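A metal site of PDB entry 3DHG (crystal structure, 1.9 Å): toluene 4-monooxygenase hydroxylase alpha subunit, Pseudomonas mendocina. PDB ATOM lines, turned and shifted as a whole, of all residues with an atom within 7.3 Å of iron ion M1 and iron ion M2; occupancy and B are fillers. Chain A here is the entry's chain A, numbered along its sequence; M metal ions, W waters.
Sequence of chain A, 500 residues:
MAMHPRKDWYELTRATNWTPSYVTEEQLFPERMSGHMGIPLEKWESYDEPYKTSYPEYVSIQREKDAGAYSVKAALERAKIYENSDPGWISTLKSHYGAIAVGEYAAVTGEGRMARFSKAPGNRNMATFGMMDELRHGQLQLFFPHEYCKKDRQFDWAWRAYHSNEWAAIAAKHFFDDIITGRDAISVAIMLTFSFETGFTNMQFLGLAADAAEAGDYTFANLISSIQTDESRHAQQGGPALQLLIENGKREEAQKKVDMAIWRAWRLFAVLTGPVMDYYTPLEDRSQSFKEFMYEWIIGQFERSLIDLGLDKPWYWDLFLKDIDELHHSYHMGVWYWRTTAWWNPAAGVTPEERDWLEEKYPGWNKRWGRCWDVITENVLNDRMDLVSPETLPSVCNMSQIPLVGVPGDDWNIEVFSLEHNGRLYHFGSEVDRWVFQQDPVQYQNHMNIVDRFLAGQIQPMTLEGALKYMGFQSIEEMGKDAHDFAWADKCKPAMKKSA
The side-chain carboxylate (OE2) of Glu 104 lies close to the side-chain amide oxygen (OE1) of Gln 141 (2.8 Å).
O of Glu 197 lies close to OG1 of Thr 201, 3.5 Å away.
O of Leu 192 sits at hydrogen-bond distance from N of Glu 197 (2.8 Å).
A ring nitrogen (ND1) of His 234 sits at hydrogen-bond distance from the side-chain carboxylate of Asp 133, 2.7 Å away.
O of His 137 lies close to OE1 of Gln 141, 3.3 Å away.
The side-chain carboxylate of Asp 230 sits at hydrogen-bond distance from a ring nitrogen (NE2) of His 137 (2.7 Å).
Of the 26 residues printed, 3 come within 4 Å of iron ion M1.
Of the 26 residues printed, 4 come within 4 Å of iron ion M2.
The nearest printed residue that does not touch iron ion M2 is His 137 (4.8 Å).
Iron ion M1 is bound by water W3 (2.0 Å), OE1 of Glu 104 (2.0 Å), OE1 of Glu 134 (2.0 Å), water W2 (2.1 Å) and ND1 of His 137 (2.3 Å).
Iron ion M1 has five donor atoms within binding distance.
Slightly farther from iron ion M1 lies water W1 (2.7 Å).
Iron ion M2 is bound by water W3 (1.9 Å), OE2 of Glu 197 (2.0 Å), OE2 of Glu 134 (2.2 Å), water W1 (2.2 Å), OE2 of Glu 231 (2.2 Å) and NE2 of His 234 (2.2 Å).
Iron ion M2 has six donor atoms within binding distance.
Water W2 bridges OE2 of Glu 104 (2.7 Å) and OE1 of Glu 231 (3.5 Å).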
ATOM      1  N   ILE A 100       7.407  14.779   0.030  1.00  0.00           N
ATOM      2  CA  ILE A 100       8.048  14.690   1.344  1.00  0.00           C
ATOM      3  C   ILE A 100       9.229  13.733   1.512  1.00  0.00           C
ATOM      4  O   ILE A 100      10.219  14.116   2.148  1.00  0.00           O
ATOM      5  CB  ILE A 100       6.991  14.521   2.497  1.00  0.00           C
ATOM      6  CG1 ILE A 100       6.096  15.773   2.607  1.00  0.00           C
ATOM      7  CG2 ILE A 100       7.667  14.137   3.845  1.00  0.00           C
ATOM      8  CD1 ILE A 100       6.833  17.112   2.915  1.00  0.00           C
ATOM      9  N   GLY A 103      12.718  14.671   0.450  1.00  0.00           N
ATOM     10  CA  GLY A 103      12.938  15.934   1.178  1.00  0.00           C
ATOM     11  C   GLY A 103      13.395  15.682   2.616  1.00  0.00           C
ATOM     12  O   GLY A 103      14.223  16.444   3.148  1.00  0.00           O
ATOM     13  N   GLU A 104      12.862  14.646   3.248  1.00  0.00           N
ATOM     14  CA  GLU A 104      13.258  14.290   4.635  1.00  0.00           C
ATOM     15  C   GLU A 104      14.704  13.843   4.583  1.00  0.00           C
ATOM     16  O   GLU A 104      15.514  14.213   5.446  1.00  0.00           O
ATOM     17  CB  GLU A 104      12.433  13.129   5.175  1.00  0.00           C
ATOM     18  CG  GLU A 104      10.965  13.407   5.322  1.00  0.00           C
ATOM     19  CD  GLU A 104      10.552  13.729   6.735  1.00  0.00           C
ATOM     20  OE1 GLU A 104      11.416  14.106   7.583  1.00  0.00           O
ATOM     21  OE2 GLU A 104       9.322  13.605   7.012  1.00  0.00           O
ATOM     22  N   TYR A 105      15.036  13.058   3.565  1.00  0.00           N
ATOM     23  CA  TYR A 105      16.434  12.658   3.357  1.00  0.00           C
ATOM     24  C   TYR A 105      17.365  13.874   3.116  1.00  0.00           C
ATOM     25  O   TYR A 105      18.459  13.920   3.672  1.00  0.00           O
ATOM     26  CB  TYR A 105      16.573  11.588   2.247  1.00  0.00           C
ATOM     27  CG  TYR A 105      17.968  11.022   2.252  1.00  0.00           C
ATOM     28  CD1 TYR A 105      18.372  10.140   3.264  1.00  0.00           C
ATOM     29  CD2 TYR A 105      18.919  11.466   1.339  1.00  0.00           C
ATOM     30  CE1 TYR A 105      19.681   9.667   3.293  1.00  0.00           C
ATOM     31  CE2 TYR A 105      20.234  10.995   1.360  1.00  0.00           C
ATOM     32  CZ  TYR A 105      20.613  10.108   2.310  1.00  0.00           C
ATOM     33  OH  TYR A 105      21.928   9.677   2.294  1.00  0.00           O
ATOM     34  N   ALA A 107      16.944  16.678   4.458  1.00  0.00           N
ATOM     35  CA  ALA A 107      17.038  17.368   5.772  1.00  0.00           C
ATOM     36  C   ALA A 107      18.231  16.831   6.579  1.00  0.00           C
ATOM     37  O   ALA A 107      18.761  17.533   7.423  1.00  0.00           O
ATOM     38  CB  ALA A 107      15.708  17.268   6.554  1.00  0.00           C
ATOM     39  N   GLU A 111      20.815  19.149   8.735  1.00  0.00           N
ATOM     40  CA  GLU A 111      21.260  18.728  10.061  1.00  0.00           C
ATOM     41  C   GLU A 111      22.798  18.532  10.094  1.00  0.00           C
ATOM     42  O   GLU A 111      23.468  19.024  10.982  1.00  0.00           O
ATOM     43  CB  GLU A 111      20.514  17.481  10.504  1.00  0.00           C
ATOM     44  CG  GLU A 111      18.978  17.745  10.821  1.00  0.00           C
ATOM     45  CD  GLU A 111      18.722  18.595  12.089  1.00  0.00           C
ATOM     46  OE1 GLU A 111      19.617  18.773  12.911  1.00  0.00           O
ATOM     47  OE2 GLU A 111      17.589  19.112  12.289  1.00  0.00           O
ATOM     48  N   GLY A 130      19.515  14.923  14.952  1.00  0.00           N
ATOM     49  CA  GLY A 130      18.663  15.342  13.809  1.00  0.00           C
ATOM     50  C   GLY A 130      19.022  14.616  12.516  1.00  0.00           C
ATOM     51  O   GLY A 130      18.103  14.247  11.709  1.00  0.00           O
ATOM     52  N   ASP A 133      17.398  11.257  12.914  1.00  0.00           N
ATOM     53  CA  ASP A 133      15.947  11.389  12.819  1.00  0.00           C
ATOM     54  C   ASP A 133      15.551  11.561  11.381  1.00  0.00           C
ATOM     55  O   ASP A 133      14.631  10.914  10.912  1.00  0.00           O
ATOM     56  CB  ASP A 133      15.423  12.623  13.569  1.00  0.00           C
ATOM     57  CG  ASP A 133      15.525  12.479  15.049  1.00  0.00           C
ATOM     58  OD1 ASP A 133      15.683  11.313  15.539  1.00  0.00           O
ATOM     59  OD2 ASP A 133      15.428  13.541  15.697  1.00  0.00           O
ATOM     60  N   GLU A 134      16.245  12.443  10.656  1.00  0.00           N
ATOM     61  CA  GLU A 134      15.766  12.654   9.254  1.00  0.00           C
ATOM     62  C   GLU A 134      16.080  11.459   8.349  1.00  0.00           C
ATOM     63  O   GLU A 134      15.329  11.181   7.415  1.00  0.00           O
ATOM     64  CB  GLU A 134      16.229  13.964   8.669  1.00  0.00           C
ATOM     65  CG  GLU A 134      15.897  15.196   9.550  1.00  0.00           C
ATOM     66  CD  GLU A 134      14.419  15.553   9.666  1.00  0.00           C
ATOM     67  OE1 GLU A 134      13.517  14.740   9.326  1.00  0.00           O
ATOM     68  OE2 GLU A 134      14.197  16.675  10.177  1.00  0.00           O
ATOM     69  N   LEU A 135      17.064  10.700   8.683  1.00  0.00           N
ATOM     70  CA  LEU A 135      17.361   9.436   8.010  1.00  0.00           C
ATOM     71  C   LEU A 135      16.229   8.431   8.196  1.00  0.00           C
ATOM     72  O   LEU A 135      15.774   7.829   7.292  1.00  0.00           O
ATOM     73  CB  LEU A 135      18.677   8.845   8.518  1.00  0.00           C
ATOM     74  CG  LEU A 135      19.077   7.491   7.936  1.00  0.00           C
ATOM     75  CD1 LEU A 135      19.300   7.584   6.436  1.00  0.00           C
ATOM     76  CD2 LEU A 135      20.315   6.951   8.638  1.00  0.00           C
ATOM     77  N   ARG A 136      15.800   8.345   9.464  1.00  0.00           N
ATOM     78  CA  ARG A 136      14.642   7.501   9.786  1.00  0.00           C
ATOM     79  C   ARG A 136      13.457   7.888   8.919  1.00  0.00           C
ATOM     80  O   ARG A 136      12.783   7.036   8.319  1.00  0.00           O
ATOM     81  CB  ARG A 136      14.259   7.654  11.263  1.00  0.00           C
ATOM     82  CG  ARG A 136      13.046   6.784  11.641  1.00  0.00           C
ATOM     83  CD  ARG A 136      12.585   7.024  13.087  1.00  0.00           C
ATOM     84  NE  ARG A 136      11.564   6.033  13.362  1.00  0.00           N
ATOM     85  CZ  ARG A 136      10.355   6.284  13.872  1.00  0.00           C
ATOM     86  NH1 ARG A 136      10.031   7.501  14.269  1.00  0.00           N
ATOM     87  NH2 ARG A 136       9.479   5.279  14.024  1.00  0.00           N
ATOM     88  N   HIS A 137      13.196   9.187   8.832  1.00  0.00           N
ATOM     89  CA  HIS A 137      11.976   9.656   8.168  1.00  0.00           C
ATOM     90  C   HIS A 137      11.996   9.417   6.676  1.00  0.00           C
ATOM     91  O   HIS A 137      11.001   8.997   6.108  1.00  0.00           O
ATOM     92  CB  HIS A 137      11.753  11.149   8.509  1.00  0.00           C
ATOM     93  CG  HIS A 137      11.574  11.356   9.975  1.00  0.00           C
ATOM     94  ND1 HIS A 137      11.567  12.610  10.573  1.00  0.00           N
ATOM     95  CD2 HIS A 137      11.356  10.459  10.975  1.00  0.00           C
ATOM     96  CE1 HIS A 137      11.395  12.454  11.883  1.00  0.00           C
ATOM     97  NE2 HIS A 137      11.262  11.164  12.153  1.00  0.00           N
ATOM     98  N   GLY A 138      13.152   9.676   6.052  1.00  0.00           N
ATOM     99  CA  GLY A 138      13.320   9.434   4.642  1.00  0.00           C
ATOM    100  C   GLY A 138      13.210   7.944   4.350  1.00  0.00           C
ATOM    101  O   GLY A 138      12.608   7.550   3.373  1.00  0.00           O
ATOM    102  N   GLN A 141       9.505   6.702   4.853  1.00  0.00           N
ATOM    103  CA  GLN A 141       8.613   7.235   3.825  1.00  0.00           C
ATOM    104  C   GLN A 141       8.989   6.815   2.424  1.00  0.00           C
ATOM    105  O   GLN A 141       8.387   7.284   1.459  1.00  0.00           O
ATOM    106  CB  GLN A 141       8.445   8.756   3.981  1.00  0.00           C
ATOM    107  CG  GLN A 141       7.681   9.005   5.294  1.00  0.00           C
ATOM    108  CD  GLN A 141       7.544  10.436   5.654  1.00  0.00           C
ATOM    109  OE1 GLN A 141       8.517  11.095   6.004  1.00  0.00           O
ATOM    110  NE2 GLN A 141       6.330  10.930   5.555  1.00  0.00           N
ATOM    111  N   LEU A 192      14.959  26.210   8.869  1.00  0.00           N
ATOM    112  CA  LEU A 192      14.413  24.892   8.886  1.00  0.00           C
ATOM    113  C   LEU A 192      13.791  24.564  10.263  1.00  0.00           C
ATOM    114  O   LEU A 192      12.619  24.195  10.329  1.00  0.00           O
ATOM    115  CB  LEU A 192      15.526  23.855   8.533  1.00  0.00           C
ATOM    116  CG  LEU A 192      15.244  22.374   8.796  1.00  0.00           C
ATOM    117  CD1 LEU A 192      14.058  21.873   7.933  1.00  0.00           C
ATOM    118  CD2 LEU A 192      16.528  21.562   8.564  1.00  0.00           C
ATOM    119  N   THR A 193      14.585  24.614  11.336  1.00  0.00           N
ATOM    120  CA  THR A 193      14.108  24.004  12.588  1.00  0.00           C
ATOM    121  C   THR A 193      13.085  24.895  13.258  1.00  0.00           C
ATOM    122  O   THR A 193      12.045  24.380  13.689  1.00  0.00           O
ATOM    123  CB  THR A 193      15.240  23.487  13.554  1.00  0.00           C
ATOM    124  OG1 THR A 193      15.875  24.597  14.226  1.00  0.00           O
ATOM    125  CG2 THR A 193      16.259  22.688  12.801  1.00  0.00           C
ATOM    126  N   PHE A 196      10.195  26.294   9.775  1.00  0.00           N
ATOM    127  CA  PHE A 196       9.452  25.245   9.083  1.00  0.00           C
ATOM    128  C   PHE A 196       8.992  24.084   9.981  1.00  0.00           C
ATOM    129  O   PHE A 196       7.838  23.749   9.996  1.00  0.00           O
ATOM    130  CB  PHE A 196      10.239  24.699   7.891  1.00  0.00           C
ATOM    131  CG  PHE A 196       9.473  23.710   7.037  1.00  0.00           C
ATOM    132  CD1 PHE A 196       8.335  24.114   6.319  1.00  0.00           C
ATOM    133  CD2 PHE A 196       9.901  22.398   6.919  1.00  0.00           C
ATOM    134  CE1 PHE A 196       7.623  23.191   5.502  1.00  0.00           C
ATOM    135  CE2 PHE A 196       9.212  21.466   6.100  1.00  0.00           C
ATOM    136  CZ  PHE A 196       8.073  21.869   5.382  1.00  0.00           C
ATOM    137  N   GLU A 197       9.924  23.457  10.688  1.00  0.00           N
ATOM    138  CA  GLU A 197       9.615  22.290  11.516  1.00  0.00           C
ATOM    139  C   GLU A 197       8.787  22.672  12.735  1.00  0.00           C
ATOM    140  O   GLU A 197       7.695  22.147  12.945  1.00  0.00           O
ATOM    141  CB  GLU A 197      10.891  21.536  11.922  1.00  0.00           C
ATOM    142  CG  GLU A 197      11.597  20.852  10.775  1.00  0.00           C
ATOM    143  CD  GLU A 197      12.928  20.219  11.162  1.00  0.00           C
ATOM    144  OE1 GLU A 197      13.749  20.818  11.893  1.00  0.00           O
ATOM    145  OE2 GLU A 197      13.152  19.103  10.712  1.00  0.00           O
ATOM    146  N   THR A 201       5.503  21.865  10.221  1.00  0.00           N
ATOM    147  CA  THR A 201       5.389  20.398  10.004  1.00  0.00           C
ATOM    148  C   THR A 201       4.925  19.685  11.258  1.00  0.00           C
ATOM    149  O   THR A 201       4.182  18.719  11.191  1.00  0.00           O
ATOM    150  CB  THR A 201       6.660  19.720   9.437  1.00  0.00           C
ATOM    151  OG1 THR A 201       7.718  19.777  10.401  1.00  0.00           O
ATOM    152  CG2 THR A 201       7.093  20.408   8.194  1.00  0.00           C
ATOM    153  N   PHE A 205       1.774  17.313  10.633  1.00  0.00           N
ATOM    154  CA  PHE A 205       1.841  15.842  10.799  1.00  0.00           C
ATOM    155  C   PHE A 205       0.811  15.359  11.810  1.00  0.00           C
ATOM    156  O   PHE A 205       0.206  14.306  11.619  1.00  0.00           O
ATOM    157  CB  PHE A 205       3.259  15.410  11.184  1.00  0.00           C
ATOM    158  CG  PHE A 205       4.152  15.187   9.997  1.00  0.00           C
ATOM    159  CD1 PHE A 205       4.135  16.091   8.926  1.00  0.00           C
ATOM    160  CD2 PHE A 205       4.987  14.080   9.917  1.00  0.00           C
ATOM    161  CE1 PHE A 205       4.952  15.901   7.800  1.00  0.00           C
ATOM    162  CE2 PHE A 205       5.801  13.874   8.773  1.00  0.00           C
ATOM    163  CZ  PHE A 205       5.783  14.782   7.726  1.00  0.00           C
ATOM    164  N   ILE A 227       6.513   9.398  13.411  1.00  0.00           N
ATOM    165  CA  ILE A 227       7.501  10.345  12.893  1.00  0.00           C
ATOM    166  C   ILE A 227       7.405  11.675  13.626  1.00  0.00           C
ATOM    167  O   ILE A 227       8.411  12.256  14.008  1.00  0.00           O
ATOM    168  CB  ILE A 227       7.292  10.523  11.385  1.00  0.00           C
ATOM    169  CG1 ILE A 227       7.827   9.289  10.677  1.00  0.00           C
ATOM    170  CG2 ILE A 227       7.996  11.790  10.853  1.00  0.00           C
ATOM    171  CD1 ILE A 227       7.460   9.248   9.150  1.00  0.00           C
ATOM    172  N   ASP A 230       9.363  12.395  16.833  1.00  0.00           N
ATOM    173  CA  ASP A 230      10.805  12.690  16.699  1.00  0.00           C
ATOM    174  C   ASP A 230      11.113  14.167  16.579  1.00  0.00           C
ATOM    175  O   ASP A 230      12.251  14.598  16.841  1.00  0.00           O
ATOM    176  CB  ASP A 230      11.407  12.001  15.469  1.00  0.00           C
ATOM    177  CG  ASP A 230      11.419  10.498  15.584  1.00  0.00           C
ATOM    178  OD1 ASP A 230      11.473   9.969  16.732  1.00  0.00           O
ATOM    179  OD2 ASP A 230      11.345   9.826  14.534  1.00  0.00           O
ATOM    180  N   GLU A 231      10.110  14.928  16.152  1.00  0.00           N
ATOM    181  CA  GLU A 231      10.303  16.291  15.678  1.00  0.00           C
ATOM    182  C   GLU A 231      10.942  17.204  16.734  1.00  0.00           C
ATOM    183  O   GLU A 231      11.966  17.810  16.473  1.00  0.00           O
ATOM    184  CB  GLU A 231       8.983  16.895  15.160  1.00  0.00           C
ATOM    185  CG  GLU A 231       9.186  18.062  14.189  1.00  0.00           C
ATOM    186  CD  GLU A 231       9.849  17.581  12.921  1.00  0.00           C
ATOM    187  OE1 GLU A 231       9.385  16.527  12.384  1.00  0.00           O
ATOM    188  OE2 GLU A 231      10.847  18.185  12.456  1.00  0.00           O
ATOM    189  N   SER A 232      10.341  17.274  17.925  1.00  0.00           N
ATOM    190  CA  SER A 232      10.787  18.238  18.946  1.00  0.00           C
ATOM    191  C   SER A 232      12.272  18.115  19.299  1.00  0.00           C
ATOM    192  O   SER A 232      12.931  19.125  19.591  1.00  0.00           O
ATOM    193  CB  SER A 232       9.921  18.136  20.200  1.00  0.00           C
ATOM    194  OG  SER A 232      10.341  17.049  21.000  1.00  0.00           O
ATOM    195  N   HIS A 234      14.903  17.647  17.466  1.00  0.00           N
ATOM    196  CA  HIS A 234      15.794  18.445  16.616  1.00  0.00           C
ATOM    197  C   HIS A 234      15.159  19.753  16.168  1.00  0.00           C
ATOM    198  O   HIS A 234      15.855  20.718  15.856  1.00  0.00           O
ATOM    199  CB  HIS A 234      16.256  17.653  15.398  1.00  0.00           C
ATOM    200  CG  HIS A 234      15.141  17.177  14.535  1.00  0.00           C
ATOM    201  ND1 HIS A 234      14.655  15.892  14.595  1.00  0.00           N
ATOM    202  CD2 HIS A 234      14.412  17.803  13.577  1.00  0.00           C
ATOM    203  CE1 HIS A 234      13.668  15.744  13.717  1.00  0.00           C
ATOM    204  NE2 HIS A 234      13.508  16.885  13.078  1.00  0.00           N
ATOM    205  N   ALA A 235      13.842  19.807  16.127  1.00  0.00           N
ATOM    206  CA  ALA A 235      13.206  21.105  15.805  1.00  0.00           C
ATOM    207  C   ALA A 235      13.517  22.217  16.826  1.00  0.00           C
ATOM    208  O   ALA A 235      13.412  23.423  16.518  1.00  0.00           O
ATOM    209  CB  ALA A 235      11.692  20.920  15.647  1.00  0.00           C
HETATM  210 FE    FE M   1      11.520  14.645   9.509  1.00  0.00          FE
HETATM  211 FE    FE M   2      12.398  17.292  11.185  1.00  0.00          FE
HETATM  212  O   HOH W   1      11.508  17.288   9.198  1.00  0.00           O
HETATM  213  O   HOH W   2       9.420  14.684   9.460  1.00  0.00           O
HETATM  214  O   HOH W   3      11.470  15.602  11.217  1.00  0.00           O
